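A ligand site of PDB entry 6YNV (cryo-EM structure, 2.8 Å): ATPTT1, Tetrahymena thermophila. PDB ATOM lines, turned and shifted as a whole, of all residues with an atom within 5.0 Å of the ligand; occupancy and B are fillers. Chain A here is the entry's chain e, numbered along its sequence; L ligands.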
ATOM      1  N   VAL A  43       2.704  -1.576  -8.255  1.00  0.00           N
ATOM      2  CA  VAL A  43       3.961  -1.883  -8.931  1.00  0.00           C
ATOM      3  C   VAL A  43       3.758  -3.196  -9.673  1.00  0.00           C
ATOM      4  O   VAL A  43       4.009  -4.287  -9.153  1.00  0.00           O
ATOM      5  CB  VAL A  43       5.130  -1.963  -7.962  1.00  0.00           C
ATOM      6  CG1 VAL A  43       6.387  -2.137  -8.728  1.00  0.00           C
ATOM      7  CG2 VAL A  43       5.194  -0.703  -7.152  1.00  0.00           C
ATOM      8  N   GLY A  44       3.312  -3.094 -10.914  1.00  0.00           N
ATOM      9  CA  GLY A  44       3.011  -4.230 -11.747  1.00  0.00           C
ATOM     10  C   GLY A  44       1.779  -3.941 -12.577  1.00  0.00           C
ATOM     11  O   GLY A  44       0.929  -3.124 -12.211  1.00  0.00           O
ATOM     12  N   ALA A  45       1.675  -4.629 -13.698  1.00  0.00           N
ATOM     13  CA  ALA A  45       0.554  -4.466 -14.599  1.00  0.00           C
ATOM     14  C   ALA A  45      -0.280  -5.719 -14.788  1.00  0.00           C
ATOM     15  O   ALA A  45      -1.477  -5.619 -15.034  1.00  0.00           O
ATOM     16  CB  ALA A  45       1.040  -3.996 -15.969  1.00  0.00           C
ATOM     17  N   ASN A  46       0.330  -6.892 -14.694  1.00  0.00           N
ATOM     18  CA  ASN A  46      -0.392  -8.126 -14.965  1.00  0.00           C
ATOM     19  C   ASN A  46      -1.477  -8.326 -13.921  1.00  0.00           C
ATOM     20  O   ASN A  46      -2.664  -8.289 -14.233  1.00  0.00           O
ATOM     21  CB  ASN A  46       0.536  -9.325 -14.972  1.00  0.00           C
ATOM     22  CG  ASN A  46      -0.157 -10.577 -15.431  1.00  0.00           C
ATOM     23  OD1 ASN A  46      -1.323 -10.562 -15.800  1.00  0.00           O
ATOM     24  ND2 ASN A  46       0.562 -11.689 -15.405  1.00  0.00           N
ATOM     25  N   LEU A  47      -1.070  -8.533 -12.669  1.00  0.00           N
ATOM     26  CA  LEU A  47      -2.003  -8.645 -11.567  1.00  0.00           C
ATOM     27  C   LEU A  47      -2.080  -7.385 -10.725  1.00  0.00           C
ATOM     28  O   LEU A  47      -3.049  -7.216  -9.982  1.00  0.00           O
ATOM     29  CB  LEU A  47      -1.606  -9.817 -10.680  1.00  0.00           C
ATOM     30  CG  LEU A  47      -2.066 -11.202 -11.097  1.00  0.00           C
ATOM     31  CD1 LEU A  47      -1.468 -12.220 -10.200  1.00  0.00           C
ATOM     32  CD2 LEU A  47      -3.558 -11.303 -11.035  1.00  0.00           C
ATOM     33  N   SER A  68       3.052   1.565 -12.198  1.00  0.00           N
ATOM     34  CA  SER A  68       4.395   1.675 -12.769  1.00  0.00           C
ATOM     35  C   SER A  68       4.963   0.291 -13.044  1.00  0.00           C
ATOM     36  O   SER A  68       5.571  -0.320 -12.164  1.00  0.00           O
ATOM     37  CB  SER A  68       5.307   2.468 -11.855  1.00  0.00           C
ATOM     38  OG  SER A  68       5.916   1.604 -10.923  1.00  0.00           O
ATOM     39  N   PHE A  69       4.774  -0.186 -14.260  1.00  0.00           N
ATOM     40  CA  PHE A  69       5.313  -1.457 -14.698  1.00  0.00           C
ATOM     41  C   PHE A  69       6.646  -1.240 -15.395  1.00  0.00           C
ATOM     42  O   PHE A  69       7.166  -0.130 -15.452  1.00  0.00           O
ATOM     43  CB  PHE A  69       4.326  -2.205 -15.587  1.00  0.00           C
ATOM     44  CG  PHE A  69       3.755  -1.388 -16.686  1.00  0.00           C
ATOM     45  CD1 PHE A  69       2.738  -0.497 -16.443  1.00  0.00           C
ATOM     46  CD2 PHE A  69       4.252  -1.493 -17.955  1.00  0.00           C
ATOM     47  CE1 PHE A  69       2.232   0.252 -17.453  1.00  0.00           C
ATOM     48  CE2 PHE A  69       3.745  -0.744 -18.965  1.00  0.00           C
ATOM     49  CZ  PHE A  69       2.730   0.128 -18.706  1.00  0.00           C
ATOM     50  N   ASP A  70       7.214  -2.313 -15.943  1.00  0.00           N
ATOM     51  CA  ASP A  70       8.601  -2.326 -16.391  1.00  0.00           C
ATOM     52  C   ASP A  70       8.715  -2.878 -17.807  1.00  0.00           C
ATOM     53  O   ASP A  70       9.603  -2.458 -18.559  1.00  0.00           O
ATOM     54  CB  ASP A  70       9.444  -3.181 -15.450  1.00  0.00           C
ATOM     55  CG  ASP A  70      10.914  -3.143 -15.797  1.00  0.00           C
ATOM     56  OD1 ASP A  70      11.337  -2.174 -16.458  1.00  0.00           O
ATOM     57  OD2 ASP A  70      11.636  -4.076 -15.411  1.00  0.00           O
ATOM     58  N   GLN A  71       7.850  -3.812 -18.169  1.00  0.00           N
ATOM     59  CA  GLN A  71       7.915  -4.436 -19.473  1.00  0.00           C
ATOM     60  C   GLN A  71       6.643  -4.153 -20.260  1.00  0.00           C
ATOM     61  O   GLN A  71       5.568  -3.992 -19.684  1.00  0.00           O
ATOM     62  CB  GLN A  71       8.133  -5.943 -19.356  1.00  0.00           C
ATOM     63  CG  GLN A  71       6.989  -6.691 -18.762  1.00  0.00           C
ATOM     64  CD  GLN A  71       7.362  -8.105 -18.389  1.00  0.00           C
ATOM     65  OE1 GLN A  71       8.540  -8.438 -18.309  1.00  0.00           O
ATOM     66  NE2 GLN A  71       6.367  -8.932 -18.147  1.00  0.00           N
ATOM     67  N   ASN A  74       2.587  -8.592 -21.853  1.00  0.00           N
ATOM     68  CA  ASN A  74       2.186  -9.626 -20.903  1.00  0.00           C
ATOM     69  C   ASN A  74       1.896 -10.901 -21.674  1.00  0.00           C
ATOM     70  O   ASN A  74       0.834 -11.046 -22.287  1.00  0.00           O
ATOM     71  CB  ASN A  74       0.966  -9.174 -20.117  1.00  0.00           C
ATOM     72  CG  ASN A  74       1.321  -8.429 -18.856  1.00  0.00           C
ATOM     73  OD1 ASN A  74       2.467  -8.456 -18.409  1.00  0.00           O
ATOM     74  ND2 ASN A  74       0.350  -7.746 -18.289  1.00  0.00           N
ATOM     75  N   TYR A  77       0.934 -16.961 -19.900  1.00  0.00           N
ATOM     76  CA  TYR A  77       1.517 -18.284 -19.714  1.00  0.00           C
ATOM     77  C   TYR A  77       0.526 -19.295 -19.170  1.00  0.00           C
ATOM     78  O   TYR A  77       0.896 -20.451 -18.967  1.00  0.00           O
ATOM     79  CB  TYR A  77       2.673 -18.195 -18.744  1.00  0.00           C
ATOM     80  CG  TYR A  77       3.715 -17.179 -19.105  1.00  0.00           C
ATOM     81  CD1 TYR A  77       4.777 -17.501 -19.912  1.00  0.00           C
ATOM     82  CD2 TYR A  77       3.661 -15.892 -18.599  1.00  0.00           C
ATOM     83  CE1 TYR A  77       5.733 -16.586 -20.225  1.00  0.00           C
ATOM     84  CE2 TYR A  77       4.613 -14.969 -18.907  1.00  0.00           C
ATOM     85  CZ  TYR A  77       5.648 -15.325 -19.729  1.00  0.00           C
ATOM     86  OH  TYR A  77       6.612 -14.405 -20.042  1.00  0.00           O
ATOM     87  N   SER A  78      -0.727 -18.913 -18.952  1.00  0.00           N
ATOM     88  CA  SER A  78      -1.742 -19.870 -18.547  1.00  0.00           C
ATOM     89  C   SER A  78      -2.179 -20.751 -19.707  1.00  0.00           C
ATOM     90  O   SER A  78      -2.686 -21.855 -19.466  1.00  0.00           O
ATOM     91  CB  SER A  78      -2.934 -19.121 -17.970  1.00  0.00           C
ATOM     92  OG  SER A  78      -2.525 -18.237 -16.954  1.00  0.00           O
ATOM     93  N   SER A  97       0.697  -4.438 -21.723  1.00  0.00           N
ATOM     94  CA  SER A  97       0.507  -4.140 -20.321  1.00  0.00           C
ATOM     95  C   SER A  97      -0.463  -2.989 -20.086  1.00  0.00           C
ATOM     96  O   SER A  97      -1.183  -2.986 -19.088  1.00  0.00           O
ATOM     97  CB  SER A  97       1.848  -3.847 -19.668  1.00  0.00           C
ATOM     98  OG  SER A  97       2.559  -5.045 -19.426  1.00  0.00           O
ATOM     99  N   LEU A 110       8.086   2.653 -16.291  1.00  0.00           N
ATOM    100  CA  LEU A 110       9.384   2.876 -15.680  1.00  0.00           C
ATOM    101  C   LEU A 110       9.492   2.043 -14.416  1.00  0.00           C
ATOM    102  O   LEU A 110       8.589   2.070 -13.562  1.00  0.00           O
ATOM    103  CB  LEU A 110       9.598   4.351 -15.358  1.00  0.00           C
ATOM    104  CG  LEU A 110       9.764   5.312 -16.522  1.00  0.00           C
ATOM    105  CD1 LEU A 110      10.199   6.655 -16.023  1.00  0.00           C
ATOM    106  CD2 LEU A 110      10.782   4.793 -17.498  1.00  0.00           C
ATOM    107  N   ALA A 111      10.594   1.315 -14.295  1.00  0.00           N
ATOM    108  CA  ALA A 111      10.859   0.502 -13.114  1.00  0.00           C
ATOM    109  C   ALA A 111      11.241   1.345 -11.918  1.00  0.00           C
ATOM    110  O   ALA A 111      11.932   2.364 -12.044  1.00  0.00           O
ATOM    111  CB  ALA A 111      11.969  -0.488 -13.427  1.00  0.00           C
ATOM    112  N   VAL A 112      10.774   0.928 -10.734  1.00  0.00           N
ATOM    113  CA  VAL A 112      11.136   1.620  -9.514  1.00  0.00           C
ATOM    114  C   VAL A 112      12.576   1.270  -9.158  1.00  0.00           C
ATOM    115  O   VAL A 112      12.938   0.098  -9.033  1.00  0.00           O
ATOM    116  CB  VAL A 112      10.159   1.284  -8.371  1.00  0.00           C
ATOM    117  CG1 VAL A 112       8.777   1.093  -8.893  1.00  0.00           C
ATOM    118  CG2 VAL A 112      10.593   0.048  -7.667  1.00  0.00           C
ATOM    119  N   ALA A 138       3.468  -6.135  -7.023  1.00  0.00           N
ATOM    120  CA  ALA A 138       3.217  -7.279  -7.884  1.00  0.00           C
ATOM    121  C   ALA A 138       4.372  -7.471  -8.842  1.00  0.00           C
ATOM    122  O   ALA A 138       4.183  -7.596 -10.056  1.00  0.00           O
ATOM    123  CB  ALA A 138       1.923  -7.106  -8.655  1.00  0.00           C
ATOM    124  N   THR A 139       5.584  -7.497  -8.317  1.00  0.00           N
ATOM    125  CA  THR A 139       6.762  -7.504  -9.159  1.00  0.00           C
ATOM    126  C   THR A 139       7.110  -8.881  -9.693  1.00  0.00           C
ATOM    127  O   THR A 139       8.136  -9.018 -10.378  1.00  0.00           O
ATOM    128  CB  THR A 139       7.948  -6.986  -8.357  1.00  0.00           C
ATOM    129  OG1 THR A 139       7.968  -7.625  -7.082  1.00  0.00           O
ATOM    130  CG2 THR A 139       7.816  -5.510  -8.150  1.00  0.00           C
ATOM    131  N   GLY A 140       6.300  -9.880  -9.417  1.00  0.00           N
ATOM    132  CA  GLY A 140       6.527 -11.200  -9.952  1.00  0.00           C
ATOM    133  C   GLY A 140       7.932 -11.718  -9.736  1.00  0.00           C
ATOM    134  O   GLY A 140       8.673 -11.208  -8.892  1.00  0.00           O
ATOM    135  N   LEU A 141       8.302 -12.738 -10.503  1.00  0.00           N
ATOM    136  CA  LEU A 141       9.648 -13.275 -10.526  1.00  0.00           C
ATOM    137  C   LEU A 141      10.281 -12.915 -11.853  1.00  0.00           C
ATOM    138  O   LEU A 141       9.803 -13.344 -12.902  1.00  0.00           O
ATOM    139  CB  LEU A 141       9.636 -14.780 -10.307  1.00  0.00           C
ATOM    140  CG  LEU A 141       9.055 -15.180  -8.964  1.00  0.00           C
ATOM    141  CD1 LEU A 141       8.400 -16.526  -9.028  1.00  0.00           C
ATOM    142  CD2 LEU A 141      10.151 -15.196  -7.955  1.00  0.00           C
ATOM    143  N   LYS A 142      11.350 -12.139 -11.796  1.00  0.00           N
ATOM    144  CA  LYS A 142      11.927 -11.582 -13.002  1.00  0.00           C
ATOM    145  C   LYS A 142      12.769 -12.623 -13.719  1.00  0.00           C
ATOM    146  O   LYS A 142      13.662 -13.237 -13.130  1.00  0.00           O
ATOM    147  CB  LYS A 142      12.763 -10.349 -12.667  1.00  0.00           C
ATOM    148  CG  LYS A 142      12.388  -9.147 -13.486  1.00  0.00           C
ATOM    149  CD  LYS A 142      13.527  -8.199 -13.669  1.00  0.00           C
ATOM    150  CE  LYS A 142      13.119  -7.028 -14.542  1.00  0.00           C
ATOM    151  NZ  LYS A 142      14.268  -6.155 -14.871  1.00  0.00           N
ATOM    152  N   HIS A 143      12.474 -12.816 -14.999  1.00  0.00           N
ATOM    153  CA  HIS A 143      13.190 -13.786 -15.809  1.00  0.00           C
ATOM    154  C   HIS A 143      14.611 -13.309 -16.080  1.00  0.00           C
ATOM    155  O   HIS A 143      14.825 -12.162 -16.482  1.00  0.00           O
ATOM    156  CB  HIS A 143      12.445 -14.008 -17.117  1.00  0.00           C
ATOM    157  CG  HIS A 143      11.250 -14.895 -16.997  1.00  0.00           C
ATOM    158  ND1 HIS A 143      10.286 -14.988 -17.982  1.00  0.00           N
ATOM    159  CD2 HIS A 143      10.855 -15.730 -16.008  1.00  0.00           C
ATOM    160  CE1 HIS A 143       9.357 -15.843 -17.604  1.00  0.00           C
ATOM    161  NE2 HIS A 143       9.678 -16.313 -16.409  1.00  0.00           N
ATOM    162  N   ASN A 165      10.227 -21.403 -22.195  1.00  0.00           N
ATOM    163  CA  ASN A 165       8.900 -21.172 -21.653  1.00  0.00           C
ATOM    164  C   ASN A 165       8.229 -19.935 -22.210  1.00  0.00           C
ATOM    165  O   ASN A 165       7.009 -19.799 -22.067  1.00  0.00           O
ATOM    166  CB  ASN A 165       8.977 -21.050 -20.134  1.00  0.00           C
ATOM    167  CG  ASN A 165       7.678 -21.327 -19.477  1.00  0.00           C
ATOM    168  OD1 ASN A 165       6.819 -21.969 -20.066  1.00  0.00           O
ATOM    169  ND2 ASN A 165       7.516 -20.843 -18.265  1.00  0.00           N
ATOM    170  N   ALA A 200       8.872 -19.321 -11.982  1.00  0.00           N
ATOM    171  CA  ALA A 200       7.529 -19.067 -12.463  1.00  0.00           C
ATOM    172  C   ALA A 200       7.105 -20.130 -13.465  1.00  0.00           C
ATOM    173  O   ALA A 200       7.877 -20.513 -14.348  1.00  0.00           O
ATOM    174  CB  ALA A 200       7.438 -17.688 -13.115  1.00  0.00           C
ATOM    175  N   GLY A 201       5.872 -20.602 -13.313  1.00  0.00           N
ATOM    176  CA  GLY A 201       5.294 -21.561 -14.226  1.00  0.00           C
ATOM    177  C   GLY A 201       5.483 -22.970 -13.754  1.00  0.00           C
ATOM    178  O   GLY A 201       5.966 -23.830 -14.504  1.00  0.00           O
ATOM    179  N   GLU A 204       1.867 -25.158 -14.783  1.00  0.00           N
ATOM    180  CA  GLU A 204       1.210 -24.705 -15.993  1.00  0.00           C
ATOM    181  C   GLU A 204       2.111 -24.761 -17.203  1.00  0.00           C
ATOM    182  O   GLU A 204       1.638 -24.582 -18.325  1.00  0.00           O
ATOM    183  CB  GLU A 204       0.700 -23.274 -15.796  1.00  0.00           C
ATOM    184  CG  GLU A 204       1.756 -22.222 -16.009  1.00  0.00           C
ATOM    185  CD  GLU A 204       1.379 -20.882 -15.412  1.00  0.00           C
ATOM    186  OE1 GLU A 204       0.216 -20.720 -14.994  1.00  0.00           O
ATOM    187  OE2 GLU A 204       2.243 -19.994 -15.368  1.00  0.00           O
ATOM    188  N   CYS A 205       3.396 -25.004 -16.996  1.00  0.00           N
ATOM    189  CA  CYS A 205       4.375 -25.031 -18.068  1.00  0.00           C
ATOM    190  C   CYS A 205       5.062 -26.387 -18.152  1.00  0.00           C
ATOM    191  O   CYS A 205       6.129 -26.502 -18.755  1.00  0.00           O
ATOM    192  CB  CYS A 205       5.383 -23.912 -17.831  1.00  0.00           C
ATOM    193  SG  CYS A 205       4.762 -22.299 -18.318  1.00  0.00           S
ATOM    194  N   GLN A 304      15.289  -9.358  -7.225  1.00  0.00           N
ATOM    195  CA  GLN A 304      15.598  -7.966  -7.469  1.00  0.00           C
ATOM    196  C   GLN A 304      16.127  -7.358  -6.183  1.00  0.00           C
ATOM    197  O   GLN A 304      15.587  -7.602  -5.108  1.00  0.00           O
ATOM    198  CB  GLN A 304      14.355  -7.220  -7.955  1.00  0.00           C
ATOM    199  CG  GLN A 304      13.538  -8.002  -8.928  1.00  0.00           C
ATOM    200  CD  GLN A 304      12.563  -7.155  -9.680  1.00  0.00           C
ATOM    201  OE1 GLN A 304      12.902  -6.091 -10.198  1.00  0.00           O
ATOM    202  NE2 GLN A 304      11.329  -7.623  -9.766  1.00  0.00           N
ATOM    203  N   PHE A 306      16.596  -4.168  -5.104  1.00  0.00           N
ATOM    204  CA  PHE A 306      15.971  -3.028  -4.453  1.00  0.00           C
ATOM    205  C   PHE A 306      14.938  -3.479  -3.428  1.00  0.00           C
ATOM    206  O   PHE A 306      14.557  -2.688  -2.566  1.00  0.00           O
ATOM    207  CB  PHE A 306      15.330  -2.111  -5.479  1.00  0.00           C
ATOM    208  CG  PHE A 306      14.114  -2.668  -6.110  1.00  0.00           C
ATOM    209  CD1 PHE A 306      14.202  -3.552  -7.164  1.00  0.00           C
ATOM    210  CD2 PHE A 306      12.863  -2.310  -5.659  1.00  0.00           C
ATOM    211  CE1 PHE A 306      13.074  -4.054  -7.749  1.00  0.00           C
ATOM    212  CE2 PHE A 306      11.738  -2.814  -6.235  1.00  0.00           C
ATOM    213  CZ  PHE A 306      11.845  -3.690  -7.282  1.00  0.00           C
ATOM    214  N   LEU A 337       1.418  -9.350  -3.665  1.00  0.00           N
ATOM    215  CA  LEU A 337       0.614 -10.423  -4.210  1.00  0.00           C
ATOM    216  C   LEU A 337       1.292 -11.042  -5.421  1.00  0.00           C
ATOM    217  O   LEU A 337       2.262 -10.515  -5.958  1.00  0.00           O
ATOM    218  CB  LEU A 337      -0.779  -9.926  -4.578  1.00  0.00           C
ATOM    219  CG  LEU A 337      -0.929  -9.243  -5.920  1.00  0.00           C
ATOM    220  CD1 LEU A 337      -2.331  -8.857  -6.124  1.00  0.00           C
ATOM    221  CD2 LEU A 337      -0.079  -8.042  -5.916  1.00  0.00           C
ATOM    222  N   GLY A 338       0.753 -12.173  -5.834  1.00  0.00           N
ATOM    223  CA  GLY A 338       1.205 -12.863  -7.022  1.00  0.00           C
ATOM    224  C   GLY A 338       2.344 -13.811  -6.742  1.00  0.00           C
ATOM    225  O   GLY A 338       2.254 -14.653  -5.857  1.00  0.00           O
ATOM    226  N   ASP A 339       3.427 -13.660  -7.506  1.00  0.00           N
ATOM    227  CA  ASP A 339       4.607 -14.497  -7.301  1.00  0.00           C
ATOM    228  C   ASP A 339       5.616 -13.854  -6.375  1.00  0.00           C
ATOM    229  O   ASP A 339       6.347 -14.570  -5.673  1.00  0.00           O
ATOM    230  CB  ASP A 339       5.248 -14.802  -8.654  1.00  0.00           C
ATOM    231  CG  ASP A 339       4.242 -15.226  -9.686  1.00  0.00           C
ATOM    232  OD1 ASP A 339       3.050 -15.308  -9.348  1.00  0.00           O
ATOM    233  OD2 ASP A 339       4.642 -15.497 -10.837  1.00  0.00           O
ATOM    234  N   ALA A 340       5.692 -12.525  -6.363  1.00  0.00           N
ATOM    235  CA  ALA A 340       6.631 -11.836  -5.489  1.00  0.00           C
ATOM    236  C   ALA A 340       6.403 -12.194  -4.030  1.00  0.00           C
ATOM    237  O   ALA A 340       7.333 -12.110  -3.223  1.00  0.00           O
ATOM    238  CB  ALA A 340       6.512 -10.329  -5.689  1.00  0.00           C
ATOM    239  N   LYS A 347       2.118 -20.813  -7.125  1.00  0.00           N
ATOM    240  CA  LYS A 347       2.022 -19.468  -7.689  1.00  0.00           C
ATOM    241  C   LYS A 347       1.343 -19.522  -9.051  1.00  0.00           C
ATOM    242  O   LYS A 347       1.984 -19.506 -10.107  1.00  0.00           O
ATOM    243  CB  LYS A 347       3.406 -18.851  -7.775  1.00  0.00           C
ATOM    244  CG  LYS A 347       4.258 -19.108  -6.573  1.00  0.00           C
ATOM    245  CD  LYS A 347       5.453 -18.198  -6.533  1.00  0.00           C
ATOM    246  CE  LYS A 347       6.151 -18.213  -5.187  1.00  0.00           C
ATOM    247  NZ  LYS A 347       5.218 -18.262  -4.033  1.00  0.00           N
ATOM    248  N   THR A 348       0.025 -19.566  -9.022  1.00  0.00           N
ATOM    249  CA  THR A 348      -0.798 -19.632 -10.226  1.00  0.00           C
ATOM    250  C   THR A 348      -1.503 -18.312 -10.453  1.00  0.00           C
ATOM    251  O   THR A 348      -1.347 -17.351  -9.697  1.00  0.00           O
ATOM    252  CB  THR A 348      -1.804 -20.778 -10.123  1.00  0.00           C
ATOM    253  OG1 THR A 348      -2.716 -20.521  -9.053  1.00  0.00           O
ATOM    254  CG2 THR A 348      -1.090 -22.053  -9.874  1.00  0.00           C
ATOM    255  N   PHE A 349      -2.280 -18.264 -11.525  1.00  0.00           N
ATOM    256  CA  PHE A 349      -3.074 -17.076 -11.821  1.00  0.00           C
ATOM    257  C   PHE A 349      -4.372 -17.076 -11.033  1.00  0.00           C
ATOM    258  O   PHE A 349      -4.742 -16.062 -10.432  1.00  0.00           O
ATOM    259  CB  PHE A 349      -3.345 -16.986 -13.314  1.00  0.00           C
ATOM    260  CG  PHE A 349      -3.827 -15.654 -13.756  1.00  0.00           C
ATOM    261  CD1 PHE A 349      -2.941 -14.679 -14.148  1.00  0.00           C
ATOM    262  CD2 PHE A 349      -5.175 -15.365 -13.799  1.00  0.00           C
ATOM    263  CE1 PHE A 349      -3.371 -13.460 -14.554  1.00  0.00           C
ATOM    264  CE2 PHE A 349      -5.610 -14.138 -14.201  1.00  0.00           C
ATOM    265  CZ  PHE A 349      -4.709 -13.185 -14.583  1.00  0.00           C
HETATM  266  P1  LIG L   1       4.543 -10.964 -13.679  1.00  0.00           P
HETATM  267  O1  LIG L   1       3.205 -10.914 -14.356  1.00  0.00           O
HETATM  268  O2  LIG L   1       5.499 -12.046 -14.095  1.00  0.00           O
HETATM  269  O3  LIG L   1       5.312  -9.495 -13.828  1.00  0.00           O
HETATM  270  C1  LIG L   1       5.030  -8.522 -12.830  1.00  0.00           C
HETATM  271  C2  LIG L   1       4.806  -7.067 -13.364  1.00  0.00           C
HETATM  272  O4  LIG L   1       5.720  -6.062 -12.493  1.00  0.00           O
HETATM  273  C3  LIG L   1       5.179  -6.917 -14.582  1.00  0.00           C
HETATM  274  O5  LIG L   1       4.412  -5.801 -15.214  1.00  0.00           O
HETATM  275  C4  LIG L   1       6.656  -6.507 -14.467  1.00  0.00           C
HETATM  276  O6  LIG L   1       7.029  -5.824 -15.583  1.00  0.00           O
HETATM  277  C5  LIG L   1       6.639  -5.567 -13.285  1.00  0.00           C
HETATM  278  N1  LIG L   1       7.951  -5.546 -12.655  1.00  0.00           N
HETATM  279  C6  LIG L   1       8.915  -6.389 -12.366  1.00  0.00           C
HETATM  280  N2  LIG L   1       9.891  -5.685 -11.760  1.00  0.00           N
HETATM  281  C7  LIG L   1       9.499  -4.400 -11.687  1.00  0.00           C
HETATM  282  C8  LIG L   1      10.128  -3.281 -11.164  1.00  0.00           C
HETATM  283  N3  LIG L   1      11.439  -3.088 -10.501  1.00  0.00           N
HETATM  284  N4  LIG L   1       9.520  -2.103 -11.214  1.00  0.00           N
HETATM  285  C9  LIG L   1       8.282  -2.007 -11.786  1.00  0.00           C
HETATM  286  N5  LIG L   1       7.663  -3.086 -12.300  1.00  0.00           N
HETATM  287  C10 LIG L   1       8.296  -4.301 -12.247  1.00  0.00           C
HETATM  288  O7  LIG L   1       4.283 -11.101 -12.066  1.00  0.00           O
HETATM  289  P2  LIG L   1       2.870 -11.735 -11.388  1.00  0.00           P
HETATM  290  O8  LIG L   1       3.210 -12.301 -10.000  1.00  0.00           O
HETATM  291  O9  LIG L   1       1.782 -10.706 -11.462  1.00  0.00           O
HETATM  292  O10 LIG L   1       2.489 -12.973 -12.371  1.00  0.00           O
HETATM  293  C11 LIG L   1       1.144 -13.341 -12.436  1.00  0.00           C
HETATM  294  C12 LIG L   1       1.012 -14.711 -13.076  1.00  0.00           C
HETATM  295  O11 LIG L   1       1.783 -14.707 -14.490  1.00  0.00           O
HETATM  296  C13 LIG L   1       1.603 -15.637 -12.376  1.00  0.00           C
HETATM  297  O12 LIG L   1       0.664 -16.190 -11.312  1.00  0.00           O
HETATM  298  C14 LIG L   1       1.914 -16.692 -13.376  1.00  0.00           C
HETATM  299  O13 LIG L   1       0.869 -17.585 -13.476  1.00  0.00           O
HETATM  300  C15 LIG L   1       2.076 -15.920 -14.728  1.00  0.00           C
HETATM  301  N6  LIG L   1       3.485 -16.026 -15.190  1.00  0.00           N
HETATM  302  C16 LIG L   1       3.953 -17.213 -15.679  1.00  0.00           C
HETATM  303  C17 LIG L   1       5.266 -17.331 -16.105  1.00  0.00           C
HETATM  304  C18 LIG L   1       5.769 -18.695 -16.682  1.00  0.00           C
HETATM  305  O14 LIG L   1       6.890 -18.807 -17.071  1.00  0.00           O
HETATM  306  N7  LIG L   1       4.815 -19.834 -16.734  1.00  0.00           N
HETATM  307  C19 LIG L   1       6.109 -16.257 -16.030  1.00  0.00           C
HETATM  308  C20 LIG L   1       5.644 -15.057 -15.538  1.00  0.00           C
HETATM  309  C21 LIG L   1       4.315 -14.950 -15.110  1.00  0.00           C
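O of Thr 348 sits at hydrogen-bond distance from O12 of the ligand (2.8 Å).
SG of Cys 205 lies within hydrogen-bond range of N7 of the ligand, 2.9 Å away.
An oxygen (O5) of the ligand lies within hydrogen-bond range of the backbone NH (N) of Ala 45, 3.3 Å away.
O14 of the ligand is in hydrogen-bond range of ND2 of Asn 165 (2.4 Å).
An oxygen (O12) of the ligand sits at hydrogen-bond distance from the side-chain carboxylate of Asp 339.
N of Val 112 is in hydrogen-bond range of N4 of the ligand, 3.3 Å away.
The side-chain amide nitrogen (NE2) of Gln 304 lies within hydrogen-bond range of a nitrogen (N2) of the ligand, 3.1 Å away.
A nitrogen (N7) of the ligand is in hydrogen-bond range of the side-chain carboxylate of Glu 204, 2.9 Å away.
The side-chain amide nitrogen (ND2) of Asn 46 sits at hydrogen-bond distance from an oxygen (O1) of the ligand, at 2.9 Å.
N of Asp 339 is in hydrogen-bond range of O8 of the ligand.
An oxygen (O6) of the ligand sits close to the backbone NH of Gln 71, at 3.4 Å.
OD2 of Asp 70 lies within salt-bridge range of NZ of Lys 142.
The side-chain sulfur (SG) of Cys 205 sits at hydrogen-bond distance from the side-chain amide oxygen (OD1) of Asn 165 (2.7 Å).
The side-chain hydroxyl (OG) of Ser 97 is in hydrogen-bond range of the backbone carbonyl oxygen (O) of Gln 71, at 3.2 Å.
N of Ala 138 sits at hydrogen-bond distance from O of Val 43.
The backbone carbonyl oxygen (O) of Phe 69 lies within hydrogen-bond range of the backbone NH (N) of Leu 110 (3.0 Å).
A nitrogen (N5) of the ligand lies close to the backbone carbonyl oxygen (O) of Ser 68, 3.5 Å away.
The backbone carbonyl oxygen (O) of Ala 138 sits close to an oxygen (O4) of the ligand (3.3 Å).
An oxygen (O14) of the ligand lies close to the backbone carbonyl oxygen (O) of Ala 200 (3.4 Å).
Val 43 touches the ligand.
CA of Gly 44 touches O4 of the ligand, 3.4 Å away.
Leu 47 touches the ligand.
Phe 69 touches the ligand (CB to O5, 3.6 Å).
N of Asp 70 touches O6 of the ligand, 3.5 Å away.
CD2 of Tyr 77 touches C16 of the ligand, 3.2 Å away.
Ala 111 touches the ligand.
Thr 139 touches the ligand (O to C6, 3.4 Å).
CA of Gly 140 touches O7 of the ligand (3.1 Å).
His 143 touches the ligand (NE2 to C19, 3.6 Å).
Gly 201 touches the ligand (CA to N7, 3.1 Å).
Phe 306 touches the ligand (CZ to N3, 3.3 Å).
Gly 338 touches the ligand.
O of Lys 347 touches O12 of the ligand, 3.8 Å away.
Phe 349 touches the ligand (N to O12, 3.6 Å).
Hydrophobic or aromatic side chains that line the ligand: Val 43, Ala 45, Leu 47, Phe 69, Tyr 77, Ala 111, His 143, Ala 200 and Phe 306.
Of the 36 residues printed, 28 come within 4 Å of the ligand.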
